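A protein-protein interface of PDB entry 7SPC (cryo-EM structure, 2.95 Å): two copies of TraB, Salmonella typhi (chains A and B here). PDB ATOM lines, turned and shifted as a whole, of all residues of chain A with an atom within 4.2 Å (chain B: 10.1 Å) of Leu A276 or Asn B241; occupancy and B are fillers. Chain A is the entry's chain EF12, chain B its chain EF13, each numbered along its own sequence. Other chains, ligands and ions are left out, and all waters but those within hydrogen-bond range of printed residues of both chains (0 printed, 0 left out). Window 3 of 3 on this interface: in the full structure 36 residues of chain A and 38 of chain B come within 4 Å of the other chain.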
ATOM      1  N   THR A 248      21.422  16.610  22.601  1.00  0.00           N
ATOM      2  CA  THR A 248      22.206  16.273  21.433  1.00  0.00           C
ATOM      3  C   THR A 248      23.385  15.328  21.780  1.00  0.00           C
ATOM      4  O   THR A 248      23.836  15.352  22.906  1.00  0.00           O
ATOM      5  CB  THR A 248      22.610  17.524  20.644  1.00  0.00           C
ATOM      6  OG1 THR A 248      23.196  18.472  21.534  1.00  0.00           O
ATOM      7  CG2 THR A 248      21.422  18.154  19.996  1.00  0.00           C
ATOM      8  N   GLY A 249      23.878  14.492  20.865  1.00  0.00           N
ATOM      9  CA  GLY A 249      24.902  13.504  21.107  1.00  0.00           C
ATOM     10  C   GLY A 249      24.442  12.290  21.872  1.00  0.00           C
ATOM     11  O   GLY A 249      25.230  11.353  22.044  1.00  0.00           O
ATOM     12  N   CYS A 250      23.198  12.271  22.341  1.00  0.00           N
ATOM     13  CA  CYS A 250      22.678  11.108  23.039  1.00  0.00           C
ATOM     14  C   CYS A 250      22.501   9.944  22.073  1.00  0.00           C
ATOM     15  O   CYS A 250      22.193  10.126  20.893  1.00  0.00           O
ATOM     16  CB  CYS A 250      21.347  11.439  23.709  1.00  0.00           C
ATOM     17  SG  CYS A 250      21.466  12.614  25.071  1.00  0.00           S
ATOM     18  N   CYS A 274      22.771   9.146  27.710  1.00  0.00           N
ATOM     19  CA  CYS A 274      23.452  10.427  27.604  1.00  0.00           C
ATOM     20  C   CYS A 274      24.518  10.529  28.682  1.00  0.00           C
ATOM     21  O   CYS A 274      24.400   9.927  29.753  1.00  0.00           O
ATOM     22  CB  CYS A 274      22.481  11.610  27.741  1.00  0.00           C
ATOM     23  SG  CYS A 274      20.998  11.514  26.711  1.00  0.00           S
ATOM     24  N   LYS A 275      25.557  11.314  28.397  1.00  0.00           N
ATOM     25  CA  LYS A 275      26.654  11.566  29.334  1.00  0.00           C
ATOM     26  C   LYS A 275      26.844  13.078  29.405  1.00  0.00           C
ATOM     27  O   LYS A 275      27.643  13.644  28.657  1.00  0.00           O
ATOM     28  CB  LYS A 275      27.928  10.855  28.894  1.00  0.00           C
ATOM     29  CG  LYS A 275      28.018   9.415  29.358  1.00  0.00           C
ATOM     30  CD  LYS A 275      29.429   8.875  29.238  1.00  0.00           C
ATOM     31  CE  LYS A 275      29.854   8.176  30.516  1.00  0.00           C
ATOM     32  NZ  LYS A 275      28.983   7.013  30.837  1.00  0.00           N
ATOM     33  N   LEU A 276      26.113  13.726  30.308  1.00  0.00           N
ATOM     34  CA  LEU A 276      26.074  15.182  30.389  1.00  0.00           C
ATOM     35  C   LEU A 276      26.635  15.627  31.734  1.00  0.00           C
ATOM     36  O   LEU A 276      25.976  15.471  32.767  1.00  0.00           O
ATOM     37  CB  LEU A 276      24.646  15.693  30.202  1.00  0.00           C
ATOM     38  CG  LEU A 276      23.793  14.967  29.165  1.00  0.00           C
ATOM     39  CD1 LEU A 276      22.317  15.097  29.498  1.00  0.00           C
ATOM     40  CD2 LEU A 276      24.077  15.502  27.774  1.00  0.00           C
ATOM     41  N   GLY A 277      27.795  16.296  31.640  1.00  0.00           N
ATOM     42  CA  GLY A 277      28.509  16.746  32.845  1.00  0.00           C
ATOM     43  C   GLY A 277      29.170  15.551  33.479  1.00  0.00           C
ATOM     44  O   GLY A 277      30.135  15.021  32.891  1.00  0.00           O
ATOM     45  N   ASP A 278      28.700  15.167  34.665  1.00  0.00           N
ATOM     46  CA  ASP A 278      29.147  13.903  35.305  1.00  0.00           C
ATOM     47  C   ASP A 278      27.845  13.134  35.505  1.00  0.00           C
ATOM     48  O   ASP A 278      27.812  12.226  36.359  1.00  0.00           O
ATOM     49  CB  ASP A 278      29.904  14.161  36.610  1.00  0.00           C
ATOM     50  CG  ASP A 278      31.253  14.837  36.416  1.00  0.00           C
ATOM     51  OD1 ASP A 278      31.890  14.593  35.373  1.00  0.00           O
ATOM     52  OD2 ASP A 278      31.652  15.605  37.311  1.00  0.00           O
ATOM     53  N   ASP A 279      26.812  13.494  34.732  1.00  0.00           N
ATOM     54  CA  ASP A 279      25.488  12.914  34.892  1.00  0.00           C
ATOM     55  C   ASP A 279      25.283  11.844  33.832  1.00  0.00           C
ATOM     56  O   ASP A 279      25.504  12.092  32.641  1.00  0.00           O
ATOM     57  CB  ASP A 279      24.398  13.984  34.788  1.00  0.00           C
ATOM     58  CG  ASP A 279      24.744  15.245  35.554  1.00  0.00           C
ATOM     59  OD1 ASP A 279      25.497  15.150  36.546  1.00  0.00           O
ATOM     60  OD2 ASP A 279      24.265  16.330  35.165  1.00  0.00           O
ATOM     61  N   TRP B 199      30.496   4.525  34.036  1.00  0.00           N
ATOM     62  CA  TRP B 199      29.345   3.776  33.552  1.00  0.00           C
ATOM     63  C   TRP B 199      29.353   3.804  32.029  1.00  0.00           C
ATOM     64  O   TRP B 199      29.206   4.870  31.422  1.00  0.00           O
ATOM     65  CB  TRP B 199      28.048   4.367  34.102  1.00  0.00           C
ATOM     66  CG  TRP B 199      26.812   3.743  33.534  1.00  0.00           C
ATOM     67  CD1 TRP B 199      26.176   4.093  32.380  1.00  0.00           C
ATOM     68  CD2 TRP B 199      26.059   2.669  34.097  1.00  0.00           C
ATOM     69  NE1 TRP B 199      25.077   3.297  32.185  1.00  0.00           N
ATOM     70  CE2 TRP B 199      24.981   2.413  33.227  1.00  0.00           C
ATOM     71  CE3 TRP B 199      26.192   1.894  35.251  1.00  0.00           C
ATOM     72  CZ2 TRP B 199      24.044   1.419  33.475  1.00  0.00           C
ATOM     73  CZ3 TRP B 199      25.260   0.908  35.495  1.00  0.00           C
ATOM     74  CH2 TRP B 199      24.197   0.677  34.612  1.00  0.00           C
ATOM     75  N   SER B 201      27.677   3.649  28.829  1.00  0.00           N
ATOM     76  CA  SER B 201      26.292   3.850  28.439  1.00  0.00           C
ATOM     77  C   SER B 201      25.897   2.892  27.322  1.00  0.00           C
ATOM     78  O   SER B 201      26.736   2.430  26.542  1.00  0.00           O
ATOM     79  CB  SER B 201      26.069   5.292  27.990  1.00  0.00           C
ATOM     80  OG  SER B 201      25.672   6.109  29.075  1.00  0.00           O
ATOM     81  N   SER B 202      24.604   2.594  27.255  1.00  0.00           N
ATOM     82  CA  SER B 202      24.091   1.723  26.209  1.00  0.00           C
ATOM     83  C   SER B 202      24.309   2.353  24.842  1.00  0.00           C
ATOM     84  O   SER B 202      24.237   3.575  24.684  1.00  0.00           O
ATOM     85  CB  SER B 202      22.605   1.449  26.430  1.00  0.00           C
ATOM     86  OG  SER B 202      22.311   1.344  27.811  1.00  0.00           O
ATOM     87  N   GLY B 203      24.582   1.513  23.851  1.00  0.00           N
ATOM     88  CA  GLY B 203      24.852   1.985  22.512  1.00  0.00           C
ATOM     89  C   GLY B 203      26.270   2.434  22.264  1.00  0.00           C
ATOM     90  O   GLY B 203      26.575   2.876  21.149  1.00  0.00           O
ATOM     91  N   SER B 204      27.148   2.344  23.261  1.00  0.00           N
ATOM     92  CA  SER B 204      28.541   2.717  23.072  1.00  0.00           C
ATOM     93  C   SER B 204      29.268   1.650  22.265  1.00  0.00           C
ATOM     94  O   SER B 204      29.057   0.451  22.454  1.00  0.00           O
ATOM     95  CB  SER B 204      29.224   2.916  24.423  1.00  0.00           C
ATOM     96  OG  SER B 204      28.405   3.680  25.288  1.00  0.00           O
ATOM     97  N   PHE B 205      30.145   2.093  21.371  1.00  0.00           N
ATOM     98  CA  PHE B 205      30.784   1.201  20.418  1.00  0.00           C
ATOM     99  C   PHE B 205      32.289   1.420  20.416  1.00  0.00           C
ATOM    100  O   PHE B 205      32.777   2.525  20.666  1.00  0.00           O
ATOM    101  CB  PHE B 205      30.217   1.402  19.008  1.00  0.00           C
ATOM    102  CG  PHE B 205      30.445   2.773  18.443  1.00  0.00           C
ATOM    103  CD1 PHE B 205      29.745   3.865  18.928  1.00  0.00           C
ATOM    104  CD2 PHE B 205      31.348   2.969  17.416  1.00  0.00           C
ATOM    105  CE1 PHE B 205      29.951   5.119  18.406  1.00  0.00           C
ATOM    106  CE2 PHE B 205      31.556   4.223  16.891  1.00  0.00           C
ATOM    107  CZ  PHE B 205      30.855   5.297  17.386  1.00  0.00           C
ATOM    108  N   VAL B 237      36.648   3.272  23.778  1.00  0.00           N
ATOM    109  CA  VAL B 237      35.226   3.047  23.776  1.00  0.00           C
ATOM    110  C   VAL B 237      34.700   4.379  23.510  1.00  0.00           C
ATOM    111  O   VAL B 237      35.102   5.292  24.156  1.00  0.00           O
ATOM    112  CB  VAL B 237      34.716   2.609  25.128  1.00  0.00           C
ATOM    113  CG1 VAL B 237      33.244   2.281  25.075  1.00  0.00           C
ATOM    114  CG2 VAL B 237      35.487   1.406  25.599  1.00  0.00           C
ATOM    115  N   GLN B 238      33.784   4.525  22.573  1.00  0.00           N
ATOM    116  CA  GLN B 238      33.264   5.812  22.212  1.00  0.00           C
ATOM    117  C   GLN B 238      31.907   5.843  22.753  1.00  0.00           C
ATOM    118  O   GLN B 238      31.138   4.977  22.474  1.00  0.00           O
ATOM    119  CB  GLN B 238      33.388   6.041  20.743  1.00  0.00           C
ATOM    120  CG  GLN B 238      34.792   6.485  20.444  1.00  0.00           C
ATOM    121  CD  GLN B 238      34.944   6.977  19.051  1.00  0.00           C
ATOM    122  OE1 GLN B 238      34.116   6.698  18.200  1.00  0.00           O
ATOM    123  NE2 GLN B 238      36.008   7.722  18.803  1.00  0.00           N
ATOM    124  N   MET B 239      31.575   6.858  23.518  1.00  0.00           N
ATOM    125  CA  MET B 239      30.347   6.868  24.260  1.00  0.00           C
ATOM    126  C   MET B 239      29.502   8.082  23.993  1.00  0.00           C
ATOM    127  O   MET B 239      29.876   8.919  23.201  1.00  0.00           O
ATOM    128  CB  MET B 239      30.693   6.792  25.745  1.00  0.00           C
ATOM    129  CG  MET B 239      31.337   5.510  26.203  1.00  0.00           C
ATOM    130  SD  MET B 239      31.685   5.562  27.955  1.00  0.00           S
ATOM    131  CE  MET B 239      32.883   6.873  28.045  1.00  0.00           C
ATOM    132  N   PRO B 240      28.319   8.167  24.596  1.00  0.00           N
ATOM    133  CA  PRO B 240      27.454   9.281  24.287  1.00  0.00           C
ATOM    134  C   PRO B 240      28.009  10.622  24.627  1.00  0.00           C
ATOM    135  O   PRO B 240      28.714  10.709  25.592  1.00  0.00           O
ATOM    136  CB  PRO B 240      26.310   9.028  25.202  1.00  0.00           C
ATOM    137  CG  PRO B 240      26.161   7.578  25.192  1.00  0.00           C
ATOM    138  CD  PRO B 240      27.565   7.104  25.278  1.00  0.00           C
ATOM    139  N   ASN B 241      27.675  11.654  23.879  1.00  0.00           N
ATOM    140  CA  ASN B 241      28.134  13.018  24.116  1.00  0.00           C
ATOM    141  C   ASN B 241      29.589  13.220  23.986  1.00  0.00           C
ATOM    142  O   ASN B 241      30.152  14.000  24.714  1.00  0.00           O
ATOM    143  CB  ASN B 241      27.658  13.559  25.431  1.00  0.00           C
ATOM    144  CG  ASN B 241      26.195  13.883  25.424  1.00  0.00           C
ATOM    145  OD1 ASN B 241      25.380  13.122  25.929  1.00  0.00           O
ATOM    146  ND2 ASN B 241      25.851  15.021  24.856  1.00  0.00           N
ATOM    147  N   ASP B 242      30.226  12.515  23.052  1.00  0.00           N
ATOM    148  CA  ASP B 242      31.672  12.668  22.805  1.00  0.00           C
ATOM    149  C   ASP B 242      32.557  12.430  24.024  1.00  0.00           C
ATOM    150  O   ASP B 242      33.461  13.220  24.293  1.00  0.00           O
ATOM    151  CB  ASP B 242      31.984  14.027  22.162  1.00  0.00           C
ATOM    152  CG  ASP B 242      31.328  14.194  20.805  1.00  0.00           C
ATOM    153  OD1 ASP B 242      30.738  13.216  20.300  1.00  0.00           O
ATOM    154  OD2 ASP B 242      31.405  15.306  20.242  1.00  0.00           O
ATOM    155  N   GLU B 243      32.306  11.353  24.761  1.00  0.00           N
ATOM    156  CA  GLU B 243      33.108  11.011  25.902  1.00  0.00           C
ATOM    157  C   GLU B 243      33.686   9.655  25.597  1.00  0.00           C
ATOM    158  O   GLU B 243      32.972   8.833  25.099  1.00  0.00           O
ATOM    159  CB  GLU B 243      32.203  10.889  27.091  1.00  0.00           C
ATOM    160  CG  GLU B 243      31.281  12.061  27.294  1.00  0.00           C
ATOM    161  CD  GLU B 243      31.924  13.162  28.101  1.00  0.00           C
ATOM    162  OE1 GLU B 243      32.716  12.837  29.005  1.00  0.00           O
ATOM    163  OE2 GLU B 243      31.627  14.348  27.845  1.00  0.00           O
ATOM    164  N   GLU B 244      34.972   9.414  25.842  1.00  0.00           N
ATOM    165  CA  GLU B 244      35.602   8.155  25.505  1.00  0.00           C
ATOM    166  C   GLU B 244      36.466   7.555  26.585  1.00  0.00           C
ATOM    167  O   GLU B 244      37.141   8.294  27.261  1.00  0.00           O
ATOM    168  CB  GLU B 244      36.388   8.314  24.241  1.00  0.00           C
ATOM    169  CG  GLU B 244      37.104   9.623  24.065  1.00  0.00           C
ATOM    170  CD  GLU B 244      37.603   9.763  22.652  1.00  0.00           C
ATOM    171  OE1 GLU B 244      37.338   8.841  21.866  1.00  0.00           O
ATOM    172  OE2 GLU B 244      38.248  10.779  22.326  1.00  0.00           O
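The side-chain sulfur (SG) of Cys A250 is disulfide-bonded to the side-chain sulfur (SG) of Cys A274.
The side-chain hydroxyl (OG) of Ser B204 lies within hydrogen-bond range of the backbone carbonyl oxygen (O) of Ser B201, at 2.4 Å.
No position is printed for both chains.
The backbone NH (N) of Lys A275 is in hydrogen-bond range of the side-chain amide oxygen (OD1) of Asn B241.
The side-chain amide nitrogen of Asn B241 lies within hydrogen-bond range of the backbone carbonyl oxygen of Thr A248, at 2.8 Å.
NZ of Lys A275 sits close to O of Trp B199 (2.2 Å).
The backbone carbonyl oxygen of Gly A249 lies within hydrogen-bond range of the backbone NH of Asn B241 (3.1 Å).
Among the printed residues, merely in contact across the chains: Gly A249 with Pro B240, Cys A274 with Pro B240, Cys A274 with Asn B241, Lys A275 with Ser B201, Lys A275 with Pro B240, Lys A275 with Glu B243 and Leu A276 with Asn B241.
Of the 14 printed residues of chain B, 5 touch a printed residue of chain A.
Printed residues of chain B that touch a printed residue of chain A: Trp B199, Ser B201, Pro B240, Asn B241 and Glu B243.
Hydrophobic or aromatic side chains of chain B that line the printed part of chain A: Pro B240.
Among the printed residues, no Asp or Glu carboxylate lies within 4 Å of a Lys or Arg side-chain nitrogen of the other chain.
Of the printed residues of chain B, Leu A276 touches Asn B241 (3.3 Å).
Asn B241 touches just these residues of chain A: Thr A248, Gly A249, Cys A274, Lys A275 and Leu A276.
Gly A249 touches just these residues of chain B: Pro B240 and Asn B241.
No residue of chain B comes within 4 Å of Gly A277.
No residue of chain B comes within 4 Å of Asp A279.
Of the printed residues of chain B, Thr A248 touches Asn B241.
Of the printed residues of chain B, Lys A275 touches Trp B199 (2.2 Å), Ser B201 (3.9 Å), Pro B240 (3.4 Å), Asn B241 (3.1 Å) and Glu B243 (3.9 Å).
Printed residues of chain A within 4 Å of Trp B199: Lys A275 (2.2 Å).
Of the printed residues of chain B, Cys A274 touches Pro B240 (3.99 Å) and Asn B241 (3.7 Å).
Printed residues of chain A within 4 Å of Pro B240: Gly A249, Cys A274 and Lys A275.
Val B237 touches none of the printed residues of chain A.
Gln B238 touches none of the printed residues of chain A.
The nearest residue of chain B that does not touch Leu A276 is Glu B243 (6.1 Å).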
